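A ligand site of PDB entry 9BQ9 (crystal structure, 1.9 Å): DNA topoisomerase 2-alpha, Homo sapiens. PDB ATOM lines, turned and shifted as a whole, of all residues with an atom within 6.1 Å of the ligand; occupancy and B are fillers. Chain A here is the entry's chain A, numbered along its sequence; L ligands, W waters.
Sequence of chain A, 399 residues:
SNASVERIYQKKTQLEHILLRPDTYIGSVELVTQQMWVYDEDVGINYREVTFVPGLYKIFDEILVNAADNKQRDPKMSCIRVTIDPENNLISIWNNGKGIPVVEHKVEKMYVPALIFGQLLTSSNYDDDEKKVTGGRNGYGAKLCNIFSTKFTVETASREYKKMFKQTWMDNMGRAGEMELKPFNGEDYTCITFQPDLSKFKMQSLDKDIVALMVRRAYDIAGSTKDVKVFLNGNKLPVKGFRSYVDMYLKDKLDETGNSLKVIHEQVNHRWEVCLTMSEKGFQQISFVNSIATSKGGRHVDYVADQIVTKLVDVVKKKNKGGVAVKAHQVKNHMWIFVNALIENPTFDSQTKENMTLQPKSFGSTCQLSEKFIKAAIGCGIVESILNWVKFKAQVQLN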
ATOM      1  N   GLN A  34       5.987 -27.566 -11.001  1.00  0.00           N
ATOM      2  CA  GLN A  34       4.642 -28.004 -10.674  1.00  0.00           C
ATOM      3  C   GLN A  34       4.334 -29.277 -11.469  1.00  0.00           C
ATOM      4  O   GLN A  34       5.017 -29.599 -12.449  1.00  0.00           O
ATOM      5  CB  GLN A  34       3.604 -26.925 -10.996  1.00  0.00           C
ATOM      6  CG  GLN A  34       3.565 -26.547 -12.464  1.00  0.00           C
ATOM      7  CD  GLN A  34       2.736 -25.314 -12.723  1.00  0.00           C
ATOM      8  OE1 GLN A  34       2.602 -24.444 -11.864  1.00  0.00           O
ATOM      9  NE2 GLN A  34       2.160 -25.218 -13.924  1.00  0.00           N
ATOM     10  N   GLN A  35       3.293 -29.980 -11.044  1.00  0.00           N
ATOM     11  CA  GLN A  35       2.885 -31.190 -11.737  1.00  0.00           C
ATOM     12  C   GLN A  35       2.081 -30.816 -12.969  1.00  0.00           C
ATOM     13  O   GLN A  35       1.187 -29.980 -12.912  1.00  0.00           O
ATOM     14  CB  GLN A  35       2.074 -32.108 -10.826  1.00  0.00           C
ATOM     15  CG  GLN A  35       2.939 -33.068 -10.036  1.00  0.00           C
ATOM     16  CD  GLN A  35       2.256 -33.568  -8.795  1.00  0.00           C
ATOM     17  OE1 GLN A  35       1.891 -32.775  -7.918  1.00  0.00           O
ATOM     18  NE2 GLN A  35       2.079 -34.877  -8.699  1.00  0.00           N
ATOM     19  N   MET A  36       2.459 -31.417 -14.100  1.00  0.00           N
ATOM     20  CA  MET A  36       1.872 -31.109 -15.396  1.00  0.00           C
ATOM     21  C   MET A  36       1.673 -32.409 -16.152  1.00  0.00           C
ATOM     22  O   MET A  36       2.283 -33.432 -15.841  1.00  0.00           O
ATOM     23  CB  MET A  36       2.774 -30.208 -16.260  1.00  0.00           C
ATOM     24  CG  MET A  36       3.223 -28.930 -15.616  1.00  0.00           C
ATOM     25  SD  MET A  36       2.016 -27.658 -15.909  1.00  0.00           S
ATOM     26  CE  MET A  36       2.289 -27.268 -17.629  1.00  0.00           C
ATOM     27  N   TRP A  37       0.823 -32.345 -17.165  1.00  0.00           N
ATOM     28  CA  TRP A  37       0.728 -33.426 -18.140  1.00  0.00           C
ATOM     29  C   TRP A  37       1.724 -33.132 -19.253  1.00  0.00           C
ATOM     30  O   TRP A  37       1.819 -31.992 -19.719  1.00  0.00           O
ATOM     31  CB  TRP A  37      -0.704 -33.549 -18.685  1.00  0.00           C
ATOM     32  CG  TRP A  37      -1.681 -34.049 -17.660  1.00  0.00           C
ATOM     33  CD1 TRP A  37      -2.488 -33.290 -16.871  1.00  0.00           C
ATOM     34  CD2 TRP A  37      -1.936 -35.417 -17.307  1.00  0.00           C
ATOM     35  NE1 TRP A  37      -3.237 -34.105 -16.056  1.00  0.00           N
ATOM     36  CE2 TRP A  37      -2.913 -35.413 -16.299  1.00  0.00           C
ATOM     37  CE3 TRP A  37      -1.420 -36.644 -17.750  1.00  0.00           C
ATOM     38  CZ2 TRP A  37      -3.400 -36.584 -15.724  1.00  0.00           C
ATOM     39  CZ3 TRP A  37      -1.904 -37.807 -17.180  1.00  0.00           C
ATOM     40  CH2 TRP A  37      -2.884 -37.767 -16.176  1.00  0.00           C
ATOM     41  N   VAL A  38       2.526 -34.129 -19.603  1.00  0.00           N
ATOM     42  CA  VAL A  38       3.522 -34.005 -20.653  1.00  0.00           C
ATOM     43  C   VAL A  38       3.490 -35.278 -21.487  1.00  0.00           C
ATOM     44  O   VAL A  38       2.900 -36.289 -21.095  1.00  0.00           O
ATOM     45  CB  VAL A  38       4.944 -33.769 -20.096  1.00  0.00           C
ATOM     46  CG1 VAL A  38       4.993 -32.493 -19.253  1.00  0.00           C
ATOM     47  CG2 VAL A  38       5.399 -34.980 -19.297  1.00  0.00           C
ATOM     48  N   TYR A  47       1.587 -37.812 -15.996  1.00  0.00           N
ATOM     49  CA  TYR A  47       1.422 -36.731 -15.031  1.00  0.00           C
ATOM     50  C   TYR A  47       2.602 -36.764 -14.079  1.00  0.00           C
ATOM     51  O   TYR A  47       2.775 -37.733 -13.329  1.00  0.00           O
ATOM     52  CB  TYR A  47       0.094 -36.907 -14.281  1.00  0.00           C
ATOM     53  CG  TYR A  47      -0.213 -35.871 -13.237  1.00  0.00           C
ATOM     54  CD1 TYR A  47      -0.681 -34.612 -13.590  1.00  0.00           C
ATOM     55  CD2 TYR A  47      -0.096 -36.177 -11.886  1.00  0.00           C
ATOM     56  CE1 TYR A  47      -0.990 -33.679 -12.621  1.00  0.00           C
ATOM     57  CE2 TYR A  47      -0.402 -35.258 -10.917  1.00  0.00           C
ATOM     58  CZ  TYR A  47      -0.851 -34.002 -11.284  1.00  0.00           C
ATOM     59  OH  TYR A  47      -1.151 -33.089 -10.305  1.00  0.00           O
ATOM     60  N   PHE A  52       9.858 -25.518 -15.788  1.00  0.00           N
ATOM     61  CA  PHE A  52       9.800 -24.860 -17.084  1.00  0.00           C
ATOM     62  C   PHE A  52       9.486 -23.390 -16.875  1.00  0.00           C
ATOM     63  O   PHE A  52       9.059 -22.965 -15.798  1.00  0.00           O
ATOM     64  CB  PHE A  52       8.754 -25.520 -17.984  1.00  0.00           C
ATOM     65  CG  PHE A  52       7.345 -25.236 -17.553  1.00  0.00           C
ATOM     66  CD1 PHE A  52       6.800 -25.890 -16.458  1.00  0.00           C
ATOM     67  CD2 PHE A  52       6.579 -24.302 -18.223  1.00  0.00           C
ATOM     68  CE1 PHE A  52       5.518 -25.626 -16.043  1.00  0.00           C
ATOM     69  CE2 PHE A  52       5.275 -24.035 -17.810  1.00  0.00           C
ATOM     70  CZ  PHE A  52       4.753 -24.685 -16.718  1.00  0.00           C
ATOM     71  N   PRO A  54       6.991 -20.563 -18.045  1.00  0.00           N
ATOM     72  CA  PRO A  54       5.719 -20.366 -18.769  1.00  0.00           C
ATOM     73  C   PRO A  54       5.829 -19.496 -20.023  1.00  0.00           C
ATOM     74  O   PRO A  54       5.284 -19.873 -21.063  1.00  0.00           O
ATOM     75  CB  PRO A  54       4.818 -19.721 -17.701  1.00  0.00           C
ATOM     76  CG  PRO A  54       5.339 -20.313 -16.404  1.00  0.00           C
ATOM     77  CD  PRO A  54       6.845 -20.381 -16.587  1.00  0.00           C
ATOM     78  N   TYR A  57       6.943 -21.524 -23.018  1.00  0.00           N
ATOM     79  CA  TYR A  57       5.865 -22.399 -23.458  1.00  0.00           C
ATOM     80  C   TYR A  57       4.817 -21.615 -24.229  1.00  0.00           C
ATOM     81  O   TYR A  57       4.258 -22.113 -25.215  1.00  0.00           O
ATOM     82  CB  TYR A  57       5.224 -23.049 -22.236  1.00  0.00           C
ATOM     83  CG  TYR A  57       4.361 -24.259 -22.484  1.00  0.00           C
ATOM     84  CD1 TYR A  57       4.431 -24.973 -23.677  1.00  0.00           C
ATOM     85  CD2 TYR A  57       3.486 -24.710 -21.510  1.00  0.00           C
ATOM     86  CE1 TYR A  57       3.654 -26.093 -23.874  1.00  0.00           C
ATOM     87  CE2 TYR A  57       2.722 -25.821 -21.690  1.00  0.00           C
ATOM     88  CZ  TYR A  57       2.794 -26.515 -22.870  1.00  0.00           C
ATOM     89  OH  TYR A  57       2.016 -27.630 -23.026  1.00  0.00           O
ATOM     90  N   LEU A 213       6.503 -30.757 -22.812  1.00  0.00           N
ATOM     91  CA  LEU A 213       5.327 -29.889 -22.795  1.00  0.00           C
ATOM     92  C   LEU A 213       4.912 -29.465 -24.199  1.00  0.00           C
ATOM     93  O   LEU A 213       3.714 -29.426 -24.520  1.00  0.00           O
ATOM     94  CB  LEU A 213       5.600 -28.655 -21.928  1.00  0.00           C
ATOM     95  CG  LEU A 213       5.533 -28.837 -20.421  1.00  0.00           C
ATOM     96  CD1 LEU A 213       6.078 -27.620 -19.686  1.00  0.00           C
ATOM     97  CD2 LEU A 213       4.067 -29.062 -20.053  1.00  0.00           C
ATOM     98  N   ARG A 216       3.299 -32.519 -25.902  1.00  0.00           N
ATOM     99  CA  ARG A 216       1.936 -32.748 -25.430  1.00  0.00           C
ATOM    100  C   ARG A 216       0.988 -31.709 -25.986  1.00  0.00           C
ATOM    101  O   ARG A 216      -0.178 -32.013 -26.262  1.00  0.00           O
ATOM    102  CB  ARG A 216       1.877 -32.729 -23.903  1.00  0.00           C
ATOM    103  CG  ARG A 216       0.636 -33.401 -23.355  1.00  0.00           C
ATOM    104  CD  ARG A 216      -0.128 -32.563 -22.352  1.00  0.00           C
ATOM    105  NE  ARG A 216      -0.623 -31.316 -22.924  1.00  0.00           N
ATOM    106  CZ  ARG A 216      -0.198 -30.103 -22.553  1.00  0.00           C
ATOM    107  NH1 ARG A 216       0.731 -29.992 -21.600  1.00  0.00           N
ATOM    108  NH2 ARG A 216      -0.716 -29.025 -23.124  1.00  0.00           N
ATOM    109  N   ARG A 217       1.473 -30.491 -26.198  1.00  0.00           N
ATOM    110  CA  ARG A 217       0.634 -29.440 -26.767  1.00  0.00           C
ATOM    111  C   ARG A 217       0.279 -29.764 -28.223  1.00  0.00           C
ATOM    112  O   ARG A 217      -0.817 -29.432 -28.694  1.00  0.00           O
ATOM    113  CB  ARG A 217       1.347 -28.088 -26.657  1.00  0.00           C
ATOM    114  CG  ARG A 217       0.475 -26.873 -26.958  1.00  0.00           C
ATOM    115  CD  ARG A 217      -0.501 -26.540 -25.825  1.00  0.00           C
ATOM    116  NE  ARG A 217      -1.361 -25.451 -26.261  1.00  0.00           N
ATOM    117  CZ  ARG A 217      -2.592 -25.643 -26.757  1.00  0.00           C
ATOM    118  NH1 ARG A 217      -3.083 -26.872 -26.842  1.00  0.00           N
ATOM    119  NH2 ARG A 217      -3.308 -24.625 -27.167  1.00  0.00           N
ATOM    120  N   ASP A 220      -2.463 -32.031 -28.010  1.00  0.00           N
ATOM    121  CA  ASP A 220      -3.668 -31.265 -27.709  1.00  0.00           C
ATOM    122  C   ASP A 220      -4.346 -30.814 -28.999  1.00  0.00           C
ATOM    123  O   ASP A 220      -5.563 -30.969 -29.158  1.00  0.00           O
ATOM    124  CB  ASP A 220      -3.351 -30.021 -26.882  1.00  0.00           C
ATOM    125  CG  ASP A 220      -2.835 -30.312 -25.484  1.00  0.00           C
ATOM    126  OD1 ASP A 220      -2.665 -31.487 -25.092  1.00  0.00           O
ATOM    127  OD2 ASP A 220      -2.595 -29.318 -24.769  1.00  0.00           O
ATOM    128  N   TYR A 245      -8.061 -38.769 -27.675  1.00  0.00           N
ATOM    129  CA  TYR A 245      -7.098 -37.971 -26.928  1.00  0.00           C
ATOM    130  C   TYR A 245      -7.307 -38.140 -25.438  1.00  0.00           C
ATOM    131  O   TYR A 245      -6.362 -38.408 -24.690  1.00  0.00           O
ATOM    132  CB  TYR A 245      -7.202 -36.502 -27.344  1.00  0.00           C
ATOM    133  CG  TYR A 245      -6.395 -35.529 -26.482  1.00  0.00           C
ATOM    134  CD1 TYR A 245      -5.041 -35.333 -26.705  1.00  0.00           C
ATOM    135  CD2 TYR A 245      -7.010 -34.801 -25.474  1.00  0.00           C
ATOM    136  CE1 TYR A 245      -4.307 -34.446 -25.920  1.00  0.00           C
ATOM    137  CE2 TYR A 245      -6.284 -33.916 -24.694  1.00  0.00           C
ATOM    138  CZ  TYR A 245      -4.938 -33.743 -24.917  1.00  0.00           C
ATOM    139  OH  TYR A 245      -4.221 -32.859 -24.142  1.00  0.00           O
ATOM    140  N   TYR A 249      -5.172 -40.148 -21.360  1.00  0.00           N
ATOM    141  CA  TYR A 249      -5.033 -39.792 -19.958  1.00  0.00           C
ATOM    142  C   TYR A 249      -5.576 -40.873 -19.034  1.00  0.00           C
ATOM    143  O   TYR A 249      -5.005 -41.140 -17.967  1.00  0.00           O
ATOM    144  CB  TYR A 249      -5.770 -38.485 -19.677  1.00  0.00           C
ATOM    145  CG  TYR A 249      -5.142 -37.244 -20.295  1.00  0.00           C
ATOM    146  CD1 TYR A 249      -5.324 -36.971 -21.646  1.00  0.00           C
ATOM    147  CD2 TYR A 249      -4.397 -36.361 -19.529  1.00  0.00           C
ATOM    148  CE1 TYR A 249      -4.761 -35.837 -22.227  1.00  0.00           C
ATOM    149  CE2 TYR A 249      -3.834 -35.228 -20.110  1.00  0.00           C
ATOM    150  CZ  TYR A 249      -4.016 -34.976 -21.456  1.00  0.00           C
ATOM    151  OH  TYR A 249      -3.463 -33.852 -22.036  1.00  0.00           O
ATOM    152  N   GLN A 284     -10.725 -31.839 -10.846  1.00  0.00           N
ATOM    153  CA  GLN A 284      -9.777 -31.706 -11.937  1.00  0.00           C
ATOM    154  C   GLN A 284     -10.515 -31.360 -13.219  1.00  0.00           C
ATOM    155  O   GLN A 284     -11.604 -31.896 -13.474  1.00  0.00           O
ATOM    156  CB  GLN A 284      -8.983 -33.000 -12.160  1.00  0.00           C
ATOM    157  CG  GLN A 284      -8.092 -33.419 -11.011  1.00  0.00           C
ATOM    158  CD  GLN A 284      -7.267 -34.642 -11.368  1.00  0.00           C
ATOM    159  OE1 GLN A 284      -6.301 -34.542 -12.131  1.00  0.00           O
ATOM    160  NE2 GLN A 284      -7.639 -35.797 -10.835  1.00  0.00           N
ATOM    161  N   GLN A 285      -9.923 -30.493 -14.036  1.00  0.00           N
ATOM    162  CA  GLN A 285     -10.484 -30.173 -15.340  1.00  0.00           C
ATOM    163  C   GLN A 285      -9.357 -30.058 -16.354  1.00  0.00           C
ATOM    164  O   GLN A 285      -8.287 -29.528 -16.044  1.00  0.00           O
ATOM    165  CB  GLN A 285     -11.305 -28.864 -15.299  1.00  0.00           C
ATOM    166  CG  GLN A 285     -10.505 -27.606 -14.971  1.00  0.00           C
ATOM    167  CD  GLN A 285      -9.903 -26.954 -16.207  1.00  0.00           C
ATOM    168  OE1 GLN A 285     -10.214 -27.343 -17.334  1.00  0.00           O
ATOM    169  NE2 GLN A 285      -9.043 -25.965 -16.003  1.00  0.00           N
ATOM    170  N   ILE A 286      -9.622 -30.563 -17.556  1.00  0.00           N
ATOM    171  CA  ILE A 286      -8.768 -30.369 -18.720  1.00  0.00           C
ATOM    172  C   ILE A 286      -9.684 -29.885 -19.840  1.00  0.00           C
ATOM    173  O   ILE A 286     -10.574 -30.619 -20.279  1.00  0.00           O
ATOM    174  CB  ILE A 286      -8.029 -31.639 -19.139  1.00  0.00           C
ATOM    175  CG1 ILE A 286      -6.922 -31.941 -18.115  1.00  0.00           C
ATOM    176  CG2 ILE A 286      -7.476 -31.487 -20.560  1.00  0.00           C
ATOM    177  CD1 ILE A 286      -6.159 -33.193 -18.396  1.00  0.00           C
ATOM    178  N   SER A 287      -9.503 -28.646 -20.277  1.00  0.00           N
ATOM    179  CA  SER A 287     -10.469 -28.027 -21.176  1.00  0.00           C
ATOM    180  C   SER A 287      -9.752 -27.257 -22.274  1.00  0.00           C
ATOM    181  O   SER A 287      -8.592 -26.851 -22.138  1.00  0.00           O
ATOM    182  CB  SER A 287     -11.400 -27.100 -20.411  1.00  0.00           C
ATOM    183  OG  SER A 287     -10.652 -26.080 -19.768  1.00  0.00           O
ATOM    184  N   PHE A 288     -10.486 -27.030 -23.369  1.00  0.00           N
ATOM    185  CA  PHE A 288     -10.003 -26.262 -24.504  1.00  0.00           C
ATOM    186  C   PHE A 288     -11.113 -25.368 -25.024  1.00  0.00           C
ATOM    187  O   PHE A 288     -12.270 -25.797 -25.121  1.00  0.00           O
ATOM    188  CB  PHE A 288      -9.514 -27.182 -25.634  1.00  0.00           C
ATOM    189  CG  PHE A 288      -8.431 -28.118 -25.200  1.00  0.00           C
ATOM    190  CD1 PHE A 288      -7.104 -27.729 -25.254  1.00  0.00           C
ATOM    191  CD2 PHE A 288      -8.734 -29.386 -24.744  1.00  0.00           C
ATOM    192  CE1 PHE A 288      -6.099 -28.576 -24.847  1.00  0.00           C
ATOM    193  CE2 PHE A 288      -7.741 -30.250 -24.331  1.00  0.00           C
ATOM    194  CZ  PHE A 288      -6.412 -29.853 -24.390  1.00  0.00           C
ATOM    195  N   ILE A 292      -7.427 -23.478 -27.561  1.00  0.00           N
ATOM    196  CA  ILE A 292      -6.593 -22.894 -26.511  1.00  0.00           C
ATOM    197  C   ILE A 292      -6.744 -23.749 -25.268  1.00  0.00           C
ATOM    198  O   ILE A 292      -7.871 -24.089 -24.881  1.00  0.00           O
ATOM    199  CB  ILE A 292      -7.000 -21.437 -26.216  1.00  0.00           C
ATOM    200  CG1 ILE A 292      -6.814 -20.556 -27.444  1.00  0.00           C
ATOM    201  CG2 ILE A 292      -6.173 -20.854 -25.049  1.00  0.00           C
ATOM    202  CD1 ILE A 292      -7.631 -19.283 -27.382  1.00  0.00           C
ATOM    203  N   ALA A 293      -5.634 -24.117 -24.649  1.00  0.00           N
ATOM    204  CA  ALA A 293      -5.669 -24.867 -23.393  1.00  0.00           C
ATOM    205  C   ALA A 293      -6.034 -23.896 -22.269  1.00  0.00           C
ATOM    206  O   ALA A 293      -5.204 -23.061 -21.871  1.00  0.00           O
ATOM    207  CB  ALA A 293      -4.332 -25.547 -23.123  1.00  0.00           C
ATOM    208  N   THR A 294      -7.270 -23.966 -21.793  1.00  0.00           N
ATOM    209  CA  THR A 294      -7.734 -23.081 -20.720  1.00  0.00           C
ATOM    210  C   THR A 294      -7.413 -23.739 -19.379  1.00  0.00           C
ATOM    211  O   THR A 294      -8.255 -24.371 -18.731  1.00  0.00           O
ATOM    212  CB  THR A 294      -9.232 -22.781 -20.877  1.00  0.00           C
ATOM    213  OG1 THR A 294      -9.927 -24.013 -21.111  1.00  0.00           O
ATOM    214  CG2 THR A 294      -9.449 -21.869 -22.073  1.00  0.00           C
ATOM    215  N   SER A 295      -6.148 -23.607 -18.971  1.00  0.00           N
ATOM    216  CA  SER A 295      -5.642 -24.315 -17.807  1.00  0.00           C
ATOM    217  C   SER A 295      -6.171 -23.781 -16.491  1.00  0.00           C
ATOM    218  O   SER A 295      -6.044 -24.459 -15.460  1.00  0.00           O
ATOM    219  CB  SER A 295      -4.097 -24.302 -17.810  1.00  0.00           C
ATOM    220  OG  SER A 295      -3.595 -22.977 -17.851  1.00  0.00           O
ATOM    221  N   LYS A 296      -6.755 -22.580 -16.478  1.00  0.00           N
ATOM    222  CA  LYS A 296      -7.427 -22.076 -15.292  1.00  0.00           C
ATOM    223  C   LYS A 296      -8.940 -22.235 -15.393  1.00  0.00           C
ATOM    224  O   LYS A 296      -9.661 -21.799 -14.495  1.00  0.00           O
ATOM    225  CB  LYS A 296      -7.049 -20.619 -15.039  1.00  0.00           C
ATOM    226  CG  LYS A 296      -5.584 -20.455 -14.584  1.00  0.00           C
ATOM    227  CD  LYS A 296      -5.240 -19.004 -14.332  1.00  0.00           C
ATOM    228  CE  LYS A 296      -3.794 -18.851 -13.881  1.00  0.00           C
ATOM    229  NZ  LYS A 296      -3.507 -19.679 -12.666  1.00  0.00           N
ATOM    230  N   GLY A 297      -9.420 -22.857 -16.469  1.00  0.00           N
ATOM    231  CA  GLY A 297     -10.832 -23.141 -16.599  1.00  0.00           C
ATOM    232  C   GLY A 297     -11.586 -22.012 -17.255  1.00  0.00           C
ATOM    233  O   GLY A 297     -11.102 -21.392 -18.210  1.00  0.00           O
ATOM    234  N   GLU A 354      -5.800 -18.329 -20.270  1.00  0.00           N
ATOM    235  CA  GLU A 354      -5.934 -19.533 -19.471  1.00  0.00           C
ATOM    236  C   GLU A 354      -7.287 -19.631 -18.778  1.00  0.00           C
ATOM    237  O   GLU A 354      -7.688 -20.732 -18.373  1.00  0.00           O
ATOM    238  CB  GLU A 354      -4.805 -19.596 -18.421  1.00  0.00           C
ATOM    239  CG  GLU A 354      -3.429 -19.576 -19.073  1.00  0.00           C
ATOM    240  CD  GLU A 354      -2.249 -19.661 -18.089  1.00  0.00           C
ATOM    241  OE1 GLU A 354      -2.467 -19.614 -16.862  1.00  0.00           O
ATOM    242  OE2 GLU A 354      -1.102 -19.772 -18.568  1.00  0.00           O
HETATM  243  C1  LIG L   1      -1.116 -25.821 -16.360  1.00  0.00           C
HETATM  244  C2  LIG L   1      -1.017 -25.820 -17.757  1.00  0.00           C
HETATM  245  C3  LIG L   1      -1.443 -27.002 -15.653  1.00  0.00           C
HETATM  246  C4  LIG L   1      -0.681 -24.690 -18.549  1.00  0.00           C
HETATM  247  C5  LIG L   1      -1.243 -27.045 -18.420  1.00  0.00           C
HETATM  248  C6  LIG L   1      -1.666 -28.210 -16.327  1.00  0.00           C
HETATM  249  C7  LIG L   1      -0.598 -24.822 -19.927  1.00  0.00           C
HETATM  250  C8  LIG L   1      -0.397 -23.334 -17.876  1.00  0.00           C
HETATM  251  C9  LIG L   1      -1.567 -28.218 -17.701  1.00  0.00           C
HETATM  252  C10 LIG L   1      -0.851 -26.042 -20.523  1.00  0.00           C
HETATM  253  C11 LIG L   1       1.164 -23.314 -17.724  1.00  0.00           C
HETATM  254  C12 LIG L   1      -1.749 -29.502 -18.552  1.00  0.00           C
HETATM  255  C13 LIG L   1      -2.402 -29.231 -14.306  1.00  0.00           C
HETATM  256  C14 LIG L   1       1.721 -22.084 -16.932  1.00  0.00           C
HETATM  257  C15 LIG L   1      -2.663 -30.610 -13.691  1.00  0.00           C
HETATM  258  C16 LIG L   1      -3.189 -30.873 -20.043  1.00  0.00           C
HETATM  259  C17 LIG L   1      -4.169 -28.947 -19.082  1.00  0.00           C
HETATM  260  C18 LIG L   1      -3.610 -30.569 -21.387  1.00  0.00           C
HETATM  261  C19 LIG L   1      -4.828 -28.425 -18.025  1.00  0.00           C
HETATM  262  C20 LIG L   1      -4.841 -28.556 -20.556  1.00  0.00           C
HETATM  263  C21 LIG L   1      -4.079 -29.211 -21.846  1.00  0.00           C
HETATM  264  C22 LIG L   1      -5.833 -27.714 -18.112  1.00  0.00           C
HETATM  265  C23 LIG L   1      -6.087 -27.657 -20.419  1.00  0.00           C
HETATM  266  C24 LIG L   1      -6.412 -27.357 -19.144  1.00  0.00           C
HETATM  267  N1  LIG L   1      -3.023 -29.814 -19.211  1.00  0.00           N
HETATM  268  O1  LIG L   1      -1.150 -27.107 -19.749  1.00  0.00           O
HETATM  269  O2  LIG L   1      -2.006 -29.413 -15.654  1.00  0.00           O
HETATM  270  O3  LIG L   1      -0.778 -26.175 -21.695  1.00  0.00           O
HETATM  271  O4  LIG L   1      -0.809 -30.216 -18.702  1.00  0.00           O
HETATM  272  O5  LIG L   1      -3.712 -31.203 -14.396  1.00  0.00           O
HETATM  273  O   HOH W   1      -5.605 -33.307 -14.236  1.00  0.00           O
HETATM  274  O   HOH W   2      -6.048 -29.249 -14.564  1.00  0.00           O
HETATM  275  O   HOH W   3      -2.538 -22.190 -15.369  1.00  0.00           O
HETATM  276  O   HOH W   4      -0.625 -23.907 -23.427  1.00  0.00           O
HETATM  277  O   HOH W   5      -2.829 -22.775 -20.575  1.00  0.00           O
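An oxygen (O3) of the ligand is in hydrogen-bond range of the guanidinium group of Arg 216 (3.2 Å). An oxygen (O4) of the ligand is in hydrogen-bond range of the backbone NH (N) of Trp 37, 3.1 Å away. NE1 of Trp 37 is in hydrogen-bond range of O5 of the ligand (3.4 Å). An oxygen (O3) of the ligand lies within hydrogen-bond range of the side-chain hydroxyl (OH) of Tyr 57 (3.4 Å).
The side-chain carboxylate (OD2) of Asp 220 lies within salt-bridge range of the guanidinium group (NH1) of Arg 217, at 3.2 Å. The backbone NH (N) of Gly 297 lies within hydrogen-bond range of the backbone carbonyl oxygen (O) of Glu 354 (3.3 Å). O of Thr 294 is in hydrogen-bond range of NE2 of Gln 285, at 3.3 Å. N of Lys 296 lies within hydrogen-bond range of O of Glu 354 (2.8 Å). NE2 of Gln 285 sits at hydrogen-bond distance from O of Ser 295, at 3.4 Å. OH of Tyr 249 is in hydrogen-bond range of OH of Tyr 245, at 2.4 Å. NE2 of Gln 34 lies within hydrogen-bond range of SD of Met 36 (3.1 Å). The guanidinium group (NH1) of Arg 216 sits at hydrogen-bond distance from the side-chain hydroxyl (OH) of Tyr 57.
Gln 35 touches the ligand (O to C13, 3.9 Å). Met 36 touches the ligand. Tyr 47 touches the ligand. Phe 52 touches the ligand. Pro 54 touches the ligand (CB to C14, 3.97 Å). Asp 220 touches the ligand (OD2 to C21, 3.3 Å). Tyr 245 touches the ligand (OH to C18, 3.6 Å). Tyr 249 touches the ligand (OH to C18, 3.3 Å). O of Gln 285 touches C22 of the ligand (3.7 Å). Ile 286 touches the ligand (CA to C24, 3.8 Å). Ser 287 touches the ligand. Phe 288 touches the ligand (CZ to C21, 3.5 Å). CB of Ala 293 touches C23 of the ligand (3.9 Å). O of Thr 294 touches C24 of the ligand, 3.5 Å away. OG of Ser 295 touches C8 of the ligand, 3.2 Å away. Glu 354 touches the ligand. 19 residues have an atom within 4 Å of the ligand: Gln 35, Met 36, Trp 37, Tyr 47, Phe 52, Pro 54, Tyr 57, Arg 216, Asp 220, Tyr 245, Tyr 249, Gln 285, Ile 286, Ser 287, Phe 288, Ala 293, Thr 294, Ser 295 and Glu 354.
Water W1 lies within hydrogen-bond range of the side-chain amide oxygen of Gln 284 (2.5 Å), an oxygen (O5) of the ligand (2.8 Å) and the indole nitrogen of Trp 37 (3.1 Å). Water W4 lies within hydrogen-bond range of O3 of the ligand (2.9 Å) and NE of Arg 217 (3.3 Å). Water W2 bridges O of Gln 285 (2.7 Å) and O5 of the ligand (3.1 Å). Water W5 bridges O of Ala 293 (2.7 Å) and OG of Ser 295 (2.8 Å). Water W3 bridges the side-chain hydroxyl (OG) of Ser 295 (2.8 Å) and the side-chain carboxylate (OE1) of Glu 354 (3.0 Å).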
